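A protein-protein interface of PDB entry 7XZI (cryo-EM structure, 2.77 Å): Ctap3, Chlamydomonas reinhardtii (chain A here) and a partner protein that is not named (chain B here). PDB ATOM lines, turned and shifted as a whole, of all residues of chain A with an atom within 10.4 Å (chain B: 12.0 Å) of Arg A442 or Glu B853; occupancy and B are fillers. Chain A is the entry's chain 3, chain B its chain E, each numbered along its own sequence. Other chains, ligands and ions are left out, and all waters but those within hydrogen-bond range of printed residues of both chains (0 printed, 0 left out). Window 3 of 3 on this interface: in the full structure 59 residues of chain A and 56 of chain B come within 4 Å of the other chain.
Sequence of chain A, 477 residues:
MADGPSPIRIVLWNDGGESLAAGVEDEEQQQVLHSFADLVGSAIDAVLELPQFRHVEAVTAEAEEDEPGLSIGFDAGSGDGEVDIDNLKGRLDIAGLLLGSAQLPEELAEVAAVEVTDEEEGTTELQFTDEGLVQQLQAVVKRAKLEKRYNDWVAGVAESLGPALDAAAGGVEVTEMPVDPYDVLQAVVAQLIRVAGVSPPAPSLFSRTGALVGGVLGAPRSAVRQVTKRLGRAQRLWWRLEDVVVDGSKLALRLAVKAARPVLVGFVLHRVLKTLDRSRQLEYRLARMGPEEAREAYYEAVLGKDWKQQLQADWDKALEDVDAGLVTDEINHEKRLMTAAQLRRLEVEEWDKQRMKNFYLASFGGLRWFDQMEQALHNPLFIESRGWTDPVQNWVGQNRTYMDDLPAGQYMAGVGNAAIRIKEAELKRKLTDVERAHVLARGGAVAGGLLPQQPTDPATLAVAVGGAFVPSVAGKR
Among the printed residues, merely in contact across the chains: Gly A416 with Tyr B847 (3.9 Å), Val A439 with Ala B851 (3.6 Å), Val A439 with Val B854 (3.6 Å), Leu A440 with Tyr B847 (3.9 Å), Arg A442 with Val B854 (3.3 Å), Gly A443 with Tyr B847 (3.6 Å) and Leu A451 with Tyr B847 (3.9 Å).
Hydrophobic or aromatic side chains of chain A that line the printed part of chain B: Val A439 and Leu A451.
Hydrophobic or aromatic side chains of chain B that line the printed part of chain A: Tyr B847, Ala B851 and Val B854.
Among the printed residues, 9 pairs touch across the chains.
OE2 of Glu B853 lies within salt-bridge range of NH1 of Arg A442, at 3.3 Å.
The backbone NH (N) of Gly A444 is in hydrogen-bond range of the side-chain hydroxyl (OH) of Tyr B847, 3.4 Å away.
Lys A423 touches none of the printed residues of chain B.
No residue of chain B comes within 4 Å of Ala A441.
Of chain B, only Glu B853 and Val B854 come within 4 Å of Arg A442.
Gly A443 touches just one residue of chain B: Tyr B847.
Gly A444 touches one residue of chain B.
No residue of chain B comes within 4 Å of Ala A445.
No residue of chain B comes within 4 Å of Val A446.
Printed residues of chain B within 4 Å of Leu A451: Tyr B847.
Arg B846 touches none of the printed residues of chain A.
Printed residues of chain A within 4 Å of Tyr B847: Gly A416, Leu A440, Gly A443, Gly A444 and Leu A451.
No residue of chain A comes within 4 Å of Ala B850.
No residue of chain A comes within 4 Å of Asp B852.
Glu B853 touches one residue of chain A.
No residue of chain A comes within 4 Å of Leu B855.
No residue of chain A comes within 4 Å of Arg B856.
The nearest residue of chain A that does not touch Glu B853 is Val A439 (6.9 Å).
The nearest printed residue of chain B that does not touch Gly A416 is Met B844 (6.6 Å).
N of Gly A449 lies within hydrogen-bond range of O of Gly A444 (2.9 Å).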
ATOM      1  N   GLY A 416     -18.208   2.707  -3.990  1.00  0.00           N
ATOM      2  CA  GLY A 416     -18.872   2.161  -5.163  1.00  0.00           C
ATOM      3  C   GLY A 416     -19.813   1.014  -4.846  1.00  0.00           C
ATOM      4  O   GLY A 416     -20.921   0.943  -5.387  1.00  0.00           O
ATOM      5  N   ILE A 420     -23.810   0.593  -5.700  1.00  0.00           N
ATOM      6  CA  ILE A 420     -24.239  -0.469  -6.607  1.00  0.00           C
ATOM      7  C   ILE A 420     -25.310  -1.327  -5.946  1.00  0.00           C
ATOM      8  O   ILE A 420     -26.321  -1.673  -6.569  1.00  0.00           O
ATOM      9  CB  ILE A 420     -23.030  -1.312  -7.061  1.00  0.00           C
ATOM     10  CG1 ILE A 420     -22.474  -0.792  -8.389  1.00  0.00           C
ATOM     11  CG2 ILE A 420     -23.407  -2.781  -7.202  1.00  0.00           C
ATOM     12  CD1 ILE A 420     -21.998   0.637  -8.348  1.00  0.00           C
ATOM     13  N   LYS A 423     -28.624   0.608  -5.744  1.00  0.00           N
ATOM     14  CA  LYS A 423     -29.301   0.648  -7.036  1.00  0.00           C
ATOM     15  C   LYS A 423     -29.870  -0.714  -7.420  1.00  0.00           C
ATOM     16  O   LYS A 423     -30.953  -0.784  -8.011  1.00  0.00           O
ATOM     17  CB  LYS A 423     -28.347   1.156  -8.118  1.00  0.00           C
ATOM     18  CG  LYS A 423     -29.009   1.380  -9.469  1.00  0.00           C
ATOM     19  CD  LYS A 423     -30.243   2.266  -9.343  1.00  0.00           C
ATOM     20  CE  LYS A 423     -29.882   3.672  -8.890  1.00  0.00           C
ATOM     21  NZ  LYS A 423     -31.090   4.518  -8.676  1.00  0.00           N
ATOM     22  N   VAL A 434     -20.835  -6.289 -17.216  1.00  0.00           N
ATOM     23  CA  VAL A 434     -20.572  -5.135 -18.071  1.00  0.00           C
ATOM     24  C   VAL A 434     -21.210  -3.875 -17.492  1.00  0.00           C
ATOM     25  O   VAL A 434     -20.596  -2.801 -17.481  1.00  0.00           O
ATOM     26  CB  VAL A 434     -21.053  -5.416 -19.507  1.00  0.00           C
ATOM     27  CG1 VAL A 434     -22.448  -6.025 -19.498  1.00  0.00           C
ATOM     28  CG2 VAL A 434     -21.026  -4.145 -20.340  1.00  0.00           C
ATOM     29  N   GLU A 435     -22.450  -3.987 -17.008  1.00  0.00           N
ATOM     30  CA  GLU A 435     -23.112  -2.838 -16.395  1.00  0.00           C
ATOM     31  C   GLU A 435     -22.355  -2.364 -15.163  1.00  0.00           C
ATOM     32  O   GLU A 435     -22.164  -1.157 -14.968  1.00  0.00           O
ATOM     33  CB  GLU A 435     -24.553  -3.199 -16.034  1.00  0.00           C
ATOM     34  CG  GLU A 435     -25.405  -3.627 -17.218  1.00  0.00           C
ATOM     35  CD  GLU A 435     -26.683  -4.323 -16.793  1.00  0.00           C
ATOM     36  OE1 GLU A 435     -26.748  -4.800 -15.640  1.00  0.00           O
ATOM     37  OE2 GLU A 435     -27.624  -4.392 -17.611  1.00  0.00           O
ATOM     38  N   ARG A 436     -21.912  -3.302 -14.323  1.00  0.00           N
ATOM     39  CA  ARG A 436     -21.137  -2.940 -13.140  1.00  0.00           C
ATOM     40  C   ARG A 436     -19.838  -2.246 -13.525  1.00  0.00           C
ATOM     41  O   ARG A 436     -19.460  -1.238 -12.916  1.00  0.00           O
ATOM     42  CB  ARG A 436     -20.851  -4.186 -12.303  1.00  0.00           C
ATOM     43  CG  ARG A 436     -19.903  -3.952 -11.139  1.00  0.00           C
ATOM     44  CD  ARG A 436     -19.504  -5.265 -10.489  1.00  0.00           C
ATOM     45  NE  ARG A 436     -20.661  -6.017 -10.025  1.00  0.00           N
ATOM     46  CZ  ARG A 436     -21.190  -5.904  -8.812  1.00  0.00           C
ATOM     47  NH1 ARG A 436     -20.684  -5.079  -7.910  1.00  0.00           N
ATOM     48  NH2 ARG A 436     -22.252  -6.640  -8.498  1.00  0.00           N
ATOM     49  N   ALA A 437     -19.142  -2.771 -14.535  1.00  0.00           N
ATOM     50  CA  ALA A 437     -17.886  -2.165 -14.963  1.00  0.00           C
ATOM     51  C   ALA A 437     -18.105  -0.752 -15.485  1.00  0.00           C
ATOM     52  O   ALA A 437     -17.351   0.165 -15.145  1.00  0.00           O
ATOM     53  CB  ALA A 437     -17.219  -3.033 -16.029  1.00  0.00           C
ATOM     54  N   HIS A 438     -19.142  -0.554 -16.305  1.00  0.00           N
ATOM     55  CA  HIS A 438     -19.419   0.780 -16.832  1.00  0.00           C
ATOM     56  C   HIS A 438     -19.790   1.753 -15.718  1.00  0.00           C
ATOM     57  O   HIS A 438     -19.328   2.902 -15.707  1.00  0.00           O
ATOM     58  CB  HIS A 438     -20.530   0.712 -17.879  1.00  0.00           C
ATOM     59  CG  HIS A 438     -20.069   0.232 -19.221  1.00  0.00           C
ATOM     60  ND1 HIS A 438     -19.571  -1.036 -19.429  1.00  0.00           N
ATOM     61  CD2 HIS A 438     -20.030   0.853 -20.424  1.00  0.00           C
ATOM     62  CE1 HIS A 438     -19.245  -1.176 -20.702  1.00  0.00           C
ATOM     63  NE2 HIS A 438     -19.514  -0.045 -21.327  1.00  0.00           N
ATOM     64  N   VAL A 439     -20.619   1.309 -14.768  1.00  0.00           N
ATOM     65  CA  VAL A 439     -21.025   2.180 -13.667  1.00  0.00           C
ATOM     66  C   VAL A 439     -19.817   2.570 -12.823  1.00  0.00           C
ATOM     67  O   VAL A 439     -19.640   3.742 -12.468  1.00  0.00           O
ATOM     68  CB  VAL A 439     -22.111   1.501 -12.815  1.00  0.00           C
ATOM     69  CG1 VAL A 439     -22.306   2.262 -11.519  1.00  0.00           C
ATOM     70  CG2 VAL A 439     -23.419   1.426 -13.580  1.00  0.00           C
ATOM     71  N   LEU A 440     -18.970   1.592 -12.487  1.00  0.00           N
ATOM     72  CA  LEU A 440     -17.782   1.887 -11.693  1.00  0.00           C
ATOM     73  C   LEU A 440     -16.834   2.814 -12.440  1.00  0.00           C
ATOM     74  O   LEU A 440     -16.243   3.721 -11.843  1.00  0.00           O
ATOM     75  CB  LEU A 440     -17.071   0.593 -11.300  1.00  0.00           C
ATOM     76  CG  LEU A 440     -17.402   0.021  -9.918  1.00  0.00           C
ATOM     77  CD1 LEU A 440     -18.842  -0.458  -9.853  1.00  0.00           C
ATOM     78  CD2 LEU A 440     -16.441  -1.099  -9.549  1.00  0.00           C
ATOM     79  N   ALA A 441     -16.675   2.603 -13.750  1.00  0.00           N
ATOM     80  CA  ALA A 441     -15.798   3.462 -14.537  1.00  0.00           C
ATOM     81  C   ALA A 441     -16.297   4.899 -14.539  1.00  0.00           C
ATOM     82  O   ALA A 441     -15.518   5.837 -14.337  1.00  0.00           O
ATOM     83  CB  ALA A 441     -15.684   2.926 -15.964  1.00  0.00           C
ATOM     84  N   ARG A 442     -17.600   5.094 -14.761  1.00  0.00           N
ATOM     85  CA  ARG A 442     -18.140   6.450 -14.769  1.00  0.00           C
ATOM     86  C   ARG A 442     -18.048   7.093 -13.390  1.00  0.00           C
ATOM     87  O   ARG A 442     -17.741   8.286 -13.275  1.00  0.00           O
ATOM     88  CB  ARG A 442     -19.583   6.451 -15.269  1.00  0.00           C
ATOM     89  CG  ARG A 442     -20.149   7.851 -15.470  1.00  0.00           C
ATOM     90  CD  ARG A 442     -21.537   7.822 -16.089  1.00  0.00           C
ATOM     91  NE  ARG A 442     -21.527   7.266 -17.436  1.00  0.00           N
ATOM     92  CZ  ARG A 442     -21.457   7.990 -18.547  1.00  0.00           C
ATOM     93  NH1 ARG A 442     -21.395   9.311 -18.510  1.00  0.00           N
ATOM     94  NH2 ARG A 442     -21.452   7.372 -19.725  1.00  0.00           N
ATOM     95  N   GLY A 443     -18.314   6.324 -12.331  1.00  0.00           N
ATOM     96  CA  GLY A 443     -18.212   6.871 -10.989  1.00  0.00           C
ATOM     97  C   GLY A 443     -16.796   7.277 -10.627  1.00  0.00           C
ATOM     98  O   GLY A 443     -16.583   8.301  -9.974  1.00  0.00           O
ATOM     99  N   GLY A 444     -15.811   6.477 -11.035  1.00  0.00           N
ATOM    100  CA  GLY A 444     -14.427   6.861 -10.816  1.00  0.00           C
ATOM    101  C   GLY A 444     -14.017   8.060 -11.648  1.00  0.00           C
ATOM    102  O   GLY A 444     -13.272   8.926 -11.180  1.00  0.00           O
ATOM    103  N   ALA A 445     -14.492   8.128 -12.894  1.00  0.00           N
ATOM    104  CA  ALA A 445     -14.124   9.235 -13.771  1.00  0.00           C
ATOM    105  C   ALA A 445     -14.709  10.554 -13.283  1.00  0.00           C
ATOM    106  O   ALA A 445     -14.046  11.595 -13.356  1.00  0.00           O
ATOM    107  CB  ALA A 445     -14.577   8.944 -15.201  1.00  0.00           C
ATOM    108  N   VAL A 446     -15.951  10.537 -12.790  1.00  0.00           N
ATOM    109  CA  VAL A 446     -16.585  11.772 -12.343  1.00  0.00           C
ATOM    110  C   VAL A 446     -15.880  12.353 -11.124  1.00  0.00           C
ATOM    111  O   VAL A 446     -15.991  13.555 -10.861  1.00  0.00           O
ATOM    112  CB  VAL A 446     -18.086  11.540 -12.062  1.00  0.00           C
ATOM    113  CG1 VAL A 446     -18.292  10.877 -10.709  1.00  0.00           C
ATOM    114  CG2 VAL A 446     -18.853  12.851 -12.147  1.00  0.00           C
ATOM    115  N   ALA A 447     -15.151  11.532 -10.373  1.00  0.00           N
ATOM    116  CA  ALA A 447     -14.384  11.995  -9.225  1.00  0.00           C
ATOM    117  C   ALA A 447     -12.917  12.229  -9.559  1.00  0.00           C
ATOM    118  O   ALA A 447     -12.135  12.568  -8.665  1.00  0.00           O
ATOM    119  CB  ALA A 447     -14.504  10.998  -8.071  1.00  0.00           C
ATOM    120  N   GLY A 448     -12.528  12.056 -10.819  1.00  0.00           N
ATOM    121  CA  GLY A 448     -11.152  12.251 -11.225  1.00  0.00           C
ATOM    122  C   GLY A 448     -10.223  11.096 -10.936  1.00  0.00           C
ATOM    123  O   GLY A 448      -9.024  11.203 -11.218  1.00  0.00           O
ATOM    124  N   GLY A 449     -10.729   9.995 -10.385  1.00  0.00           N
ATOM    125  CA  GLY A 449      -9.901   8.858 -10.051  1.00  0.00           C
ATOM    126  C   GLY A 449      -9.092   9.004  -8.782  1.00  0.00           C
ATOM    127  O   GLY A 449      -8.276   8.123  -8.484  1.00  0.00           O
ATOM    128  N   LEU A 450      -9.288  10.085  -8.025  1.00  0.00           N
ATOM    129  CA  LEU A 450      -8.526  10.303  -6.802  1.00  0.00           C
ATOM    130  C   LEU A 450      -9.080   9.532  -5.611  1.00  0.00           C
ATOM    131  O   LEU A 450      -8.422   9.480  -4.567  1.00  0.00           O
ATOM    132  CB  LEU A 450      -8.483  11.797  -6.474  1.00  0.00           C
ATOM    133  CG  LEU A 450      -7.885  12.705  -7.549  1.00  0.00           C
ATOM    134  CD1 LEU A 450      -7.973  14.162  -7.128  1.00  0.00           C
ATOM    135  CD2 LEU A 450      -6.446  12.317  -7.842  1.00  0.00           C
ATOM    136  N   LEU A 451     -10.267   8.946  -5.737  1.00  0.00           N
ATOM    137  CA  LEU A 451     -10.843   8.198  -4.629  1.00  0.00           C
ATOM    138  C   LEU A 451     -10.016   6.944  -4.358  1.00  0.00           C
ATOM    139  O   LEU A 451      -9.462   6.349  -5.289  1.00  0.00           O
ATOM    140  CB  LEU A 451     -12.293   7.818  -4.931  1.00  0.00           C
ATOM    141  CG  LEU A 451     -13.322   8.942  -4.801  1.00  0.00           C
ATOM    142  CD1 LEU A 451     -14.707   8.453  -5.191  1.00  0.00           C
ATOM    143  CD2 LEU A 451     -13.325   9.490  -3.383  1.00  0.00           C
ATOM    144  N   ASN B 842     -21.690  12.331   0.317  1.00  0.00           N
ATOM    145  CA  ASN B 842     -21.681  13.048  -0.958  1.00  0.00           C
ATOM    146  C   ASN B 842     -21.090  12.186  -2.071  1.00  0.00           C
ATOM    147  O   ASN B 842     -21.603  12.162  -3.199  1.00  0.00           O
ATOM    148  CB  ASN B 842     -20.906  14.359  -0.824  1.00  0.00           C
ATOM    149  CG  ASN B 842     -21.608  15.363   0.066  1.00  0.00           C
ATOM    150  OD1 ASN B 842     -22.834  15.358   0.183  1.00  0.00           O
ATOM    151  ND2 ASN B 842     -20.833  16.235   0.700  1.00  0.00           N
ATOM    152  N   ALA B 843     -20.001  11.474  -1.771  1.00  0.00           N
ATOM    153  CA  ALA B 843     -19.396  10.594  -2.767  1.00  0.00           C
ATOM    154  C   ALA B 843     -20.357   9.486  -3.180  1.00  0.00           C
ATOM    155  O   ALA B 843     -20.472   9.161  -4.369  1.00  0.00           O
ATOM    156  CB  ALA B 843     -18.096  10.004  -2.223  1.00  0.00           C
ATOM    157  N   MET B 844     -21.059   8.895  -2.211  1.00  0.00           N
ATOM    158  CA  MET B 844     -22.026   7.850  -2.528  1.00  0.00           C
ATOM    159  C   MET B 844     -23.179   8.401  -3.357  1.00  0.00           C
ATOM    160  O   MET B 844     -23.683   7.722  -4.257  1.00  0.00           O
ATOM    161  CB  MET B 844     -22.547   7.205  -1.245  1.00  0.00           C
ATOM    162  CG  MET B 844     -23.387   5.960  -1.484  1.00  0.00           C
ATOM    163  SD  MET B 844     -24.062   5.259   0.032  1.00  0.00           S
ATOM    164  CE  MET B 844     -25.106   6.602   0.593  1.00  0.00           C
ATOM    165  N   ALA B 845     -23.617   9.627  -3.063  1.00  0.00           N
ATOM    166  CA  ALA B 845     -24.679  10.240  -3.856  1.00  0.00           C
ATOM    167  C   ALA B 845     -24.236  10.458  -5.298  1.00  0.00           C
ATOM    168  O   ALA B 845     -25.002  10.211  -6.237  1.00  0.00           O
ATOM    169  CB  ALA B 845     -25.115  11.559  -3.221  1.00  0.00           C
ATOM    170  N   ARG B 846     -22.998  10.921  -5.494  1.00  0.00           N
ATOM    171  CA  ARG B 846     -22.484  11.087  -6.852  1.00  0.00           C
ATOM    172  C   ARG B 846     -22.385   9.747  -7.575  1.00  0.00           C
ATOM    173  O   ARG B 846     -22.709   9.646  -8.767  1.00  0.00           O
ATOM    174  CB  ARG B 846     -21.125  11.786  -6.825  1.00  0.00           C
ATOM    175  CG  ARG B 846     -21.208  13.286  -6.599  1.00  0.00           C
ATOM    176  CD  ARG B 846     -19.865  13.957  -6.832  1.00  0.00           C
ATOM    177  NE  ARG B 846     -18.902  13.637  -5.789  1.00  0.00           N
ATOM    178  CZ  ARG B 846     -18.717  14.364  -4.693  1.00  0.00           C
ATOM    179  NH1 ARG B 846     -19.420  15.462  -4.465  1.00  0.00           N
ATOM    180  NH2 ARG B 846     -17.804  13.981  -3.806  1.00  0.00           N
ATOM    181  N   TYR B 847     -21.935   8.706  -6.870  1.00  0.00           N
ATOM    182  CA  TYR B 847     -21.877   7.377  -7.472  1.00  0.00           C
ATOM    183  C   TYR B 847     -23.266   6.885  -7.862  1.00  0.00           C
ATOM    184  O   TYR B 847     -23.444   6.278  -8.923  1.00  0.00           O
ATOM    185  CB  TYR B 847     -21.210   6.390  -6.514  1.00  0.00           C
ATOM    186  CG  TYR B 847     -19.820   5.973  -6.936  1.00  0.00           C
ATOM    187  CD1 TYR B 847     -19.629   4.908  -7.804  1.00  0.00           C
ATOM    188  CD2 TYR B 847     -18.702   6.643  -6.464  1.00  0.00           C
ATOM    189  CE1 TYR B 847     -18.361   4.521  -8.190  1.00  0.00           C
ATOM    190  CE2 TYR B 847     -17.429   6.263  -6.845  1.00  0.00           C
ATOM    191  CZ  TYR B 847     -17.265   5.203  -7.708  1.00  0.00           C
ATOM    192  OH  TYR B 847     -16.000   4.823  -8.089  1.00  0.00           O
ATOM    193  N   LEU B 848     -24.263   7.130  -7.008  1.00  0.00           N
ATOM    194  CA  LEU B 848     -25.633   6.746  -7.328  1.00  0.00           C
ATOM    195  C   LEU B 848     -26.147   7.499  -8.547  1.00  0.00           C
ATOM    196  O   LEU B 848     -26.854   6.928  -9.386  1.00  0.00           O
ATOM    197  CB  LEU B 848     -26.545   6.988  -6.126  1.00  0.00           C
ATOM    198  CG  LEU B 848     -26.571   5.901  -5.054  1.00  0.00           C
ATOM    199  CD1 LEU B 848     -27.477   6.306  -3.902  1.00  0.00           C
ATOM    200  CD2 LEU B 848     -27.028   4.586  -5.661  1.00  0.00           C
ATOM    201  N   ALA B 849     -25.822   8.789  -8.652  1.00  0.00           N
ATOM    202  CA  ALA B 849     -26.225   9.554  -9.827  1.00  0.00           C
ATOM    203  C   ALA B 849     -25.596   8.985 -11.094  1.00  0.00           C
ATOM    204  O   ALA B 849     -26.266   8.850 -12.127  1.00  0.00           O
ATOM    205  CB  ALA B 849     -25.848  11.025  -9.651  1.00  0.00           C
ATOM    206  N   ALA B 850     -24.309   8.635 -11.029  1.00  0.00           N
ATOM    207  CA  ALA B 850     -23.650   8.030 -12.182  1.00  0.00           C
ATOM    208  C   ALA B 850     -24.286   6.691 -12.543  1.00  0.00           C
ATOM    209  O   ALA B 850     -24.480   6.383 -13.726  1.00  0.00           O
ATOM    210  CB  ALA B 850     -22.157   7.857 -11.903  1.00  0.00           C
ATOM    211  N   ALA B 851     -24.612   5.880 -11.534  1.00  0.00           N
ATOM    212  CA  ALA B 851     -25.255   4.594 -11.786  1.00  0.00           C
ATOM    213  C   ALA B 851     -26.618   4.777 -12.438  1.00  0.00           C
ATOM    214  O   ALA B 851     -26.981   4.030 -13.355  1.00  0.00           O
ATOM    215  CB  ALA B 851     -25.386   3.810 -10.482  1.00  0.00           C
ATOM    216  N   ASP B 852     -27.393   5.757 -11.969  1.00  0.00           N
ATOM    217  CA  ASP B 852     -28.693   6.027 -12.573  1.00  0.00           C
ATOM    218  C   ASP B 852     -28.542   6.485 -14.017  1.00  0.00           C
ATOM    219  O   ASP B 852     -29.344   6.112 -14.881  1.00  0.00           O
ATOM    220  CB  ASP B 852     -29.450   7.074 -11.757  1.00  0.00           C
ATOM    221  CG  ASP B 852     -30.822   7.374 -12.328  1.00  0.00           C
ATOM    222  OD1 ASP B 852     -31.712   6.503 -12.227  1.00  0.00           O
ATOM    223  OD2 ASP B 852     -31.011   8.478 -12.881  1.00  0.00           O
ATOM    224  N   GLU B 853     -27.527   7.307 -14.295  1.00  0.00           N
ATOM    225  CA  GLU B 853     -27.287   7.732 -15.671  1.00  0.00           C
ATOM    226  C   GLU B 853     -26.937   6.544 -16.560  1.00  0.00           C
ATOM    227  O   GLU B 853     -27.431   6.431 -17.688  1.00  0.00           O
ATOM    228  CB  GLU B 853     -26.176   8.780 -15.717  1.00  0.00           C
ATOM    229  CG  GLU B 853     -25.859   9.267 -17.123  1.00  0.00           C
ATOM    230  CD  GLU B 853     -24.674  10.211 -17.164  1.00  0.00           C
ATOM    231  OE1 GLU B 853     -24.061  10.445 -16.103  1.00  0.00           O
ATOM    232  OE2 GLU B 853     -24.356  10.719 -18.260  1.00  0.00           O
ATOM    233  N   VAL B 854     -26.084   5.644 -16.066  1.00  0.00           N
ATOM    234  CA  VAL B 854     -25.652   4.509 -16.880  1.00  0.00           C
ATOM    235  C   VAL B 854     -26.810   3.550 -17.129  1.00  0.00           C
ATOM    236  O   VAL B 854     -27.052   3.125 -18.266  1.00  0.00           O
ATOM    237  CB  VAL B 854     -24.463   3.789 -16.217  1.00  0.00           C
ATOM    238  CG1 VAL B 854     -24.127   2.519 -16.980  1.00  0.00           C
ATOM    239  CG2 VAL B 854     -23.256   4.701 -16.166  1.00  0.00           C
ATOM    240  N   LEU B 855     -27.546   3.196 -16.074  1.00  0.00           N
ATOM    241  CA  LEU B 855     -28.573   2.167 -16.182  1.00  0.00           C
ATOM    242  C   LEU B 855     -29.800   2.620 -16.962  1.00  0.00           C
ATOM    243  O   LEU B 855     -30.623   1.773 -17.327  1.00  0.00           O
ATOM    244  CB  LEU B 855     -28.997   1.702 -14.787  1.00  0.00           C
ATOM    245  N   ARG B 856     -29.944   3.913 -17.228  1.00  0.00           N
ATOM    246  CA  ARG B 856     -31.098   4.412 -17.966  1.00  0.00           C
ATOM    247  C   ARG B 856     -30.727   5.615 -18.825  1.00  0.00           C
ATOM    248  O   ARG B 856     -31.338   5.857 -19.866  1.00  0.00           O
ATOM    249  CB  ARG B 856     -32.229   4.782 -17.002  1.00  0.00           C
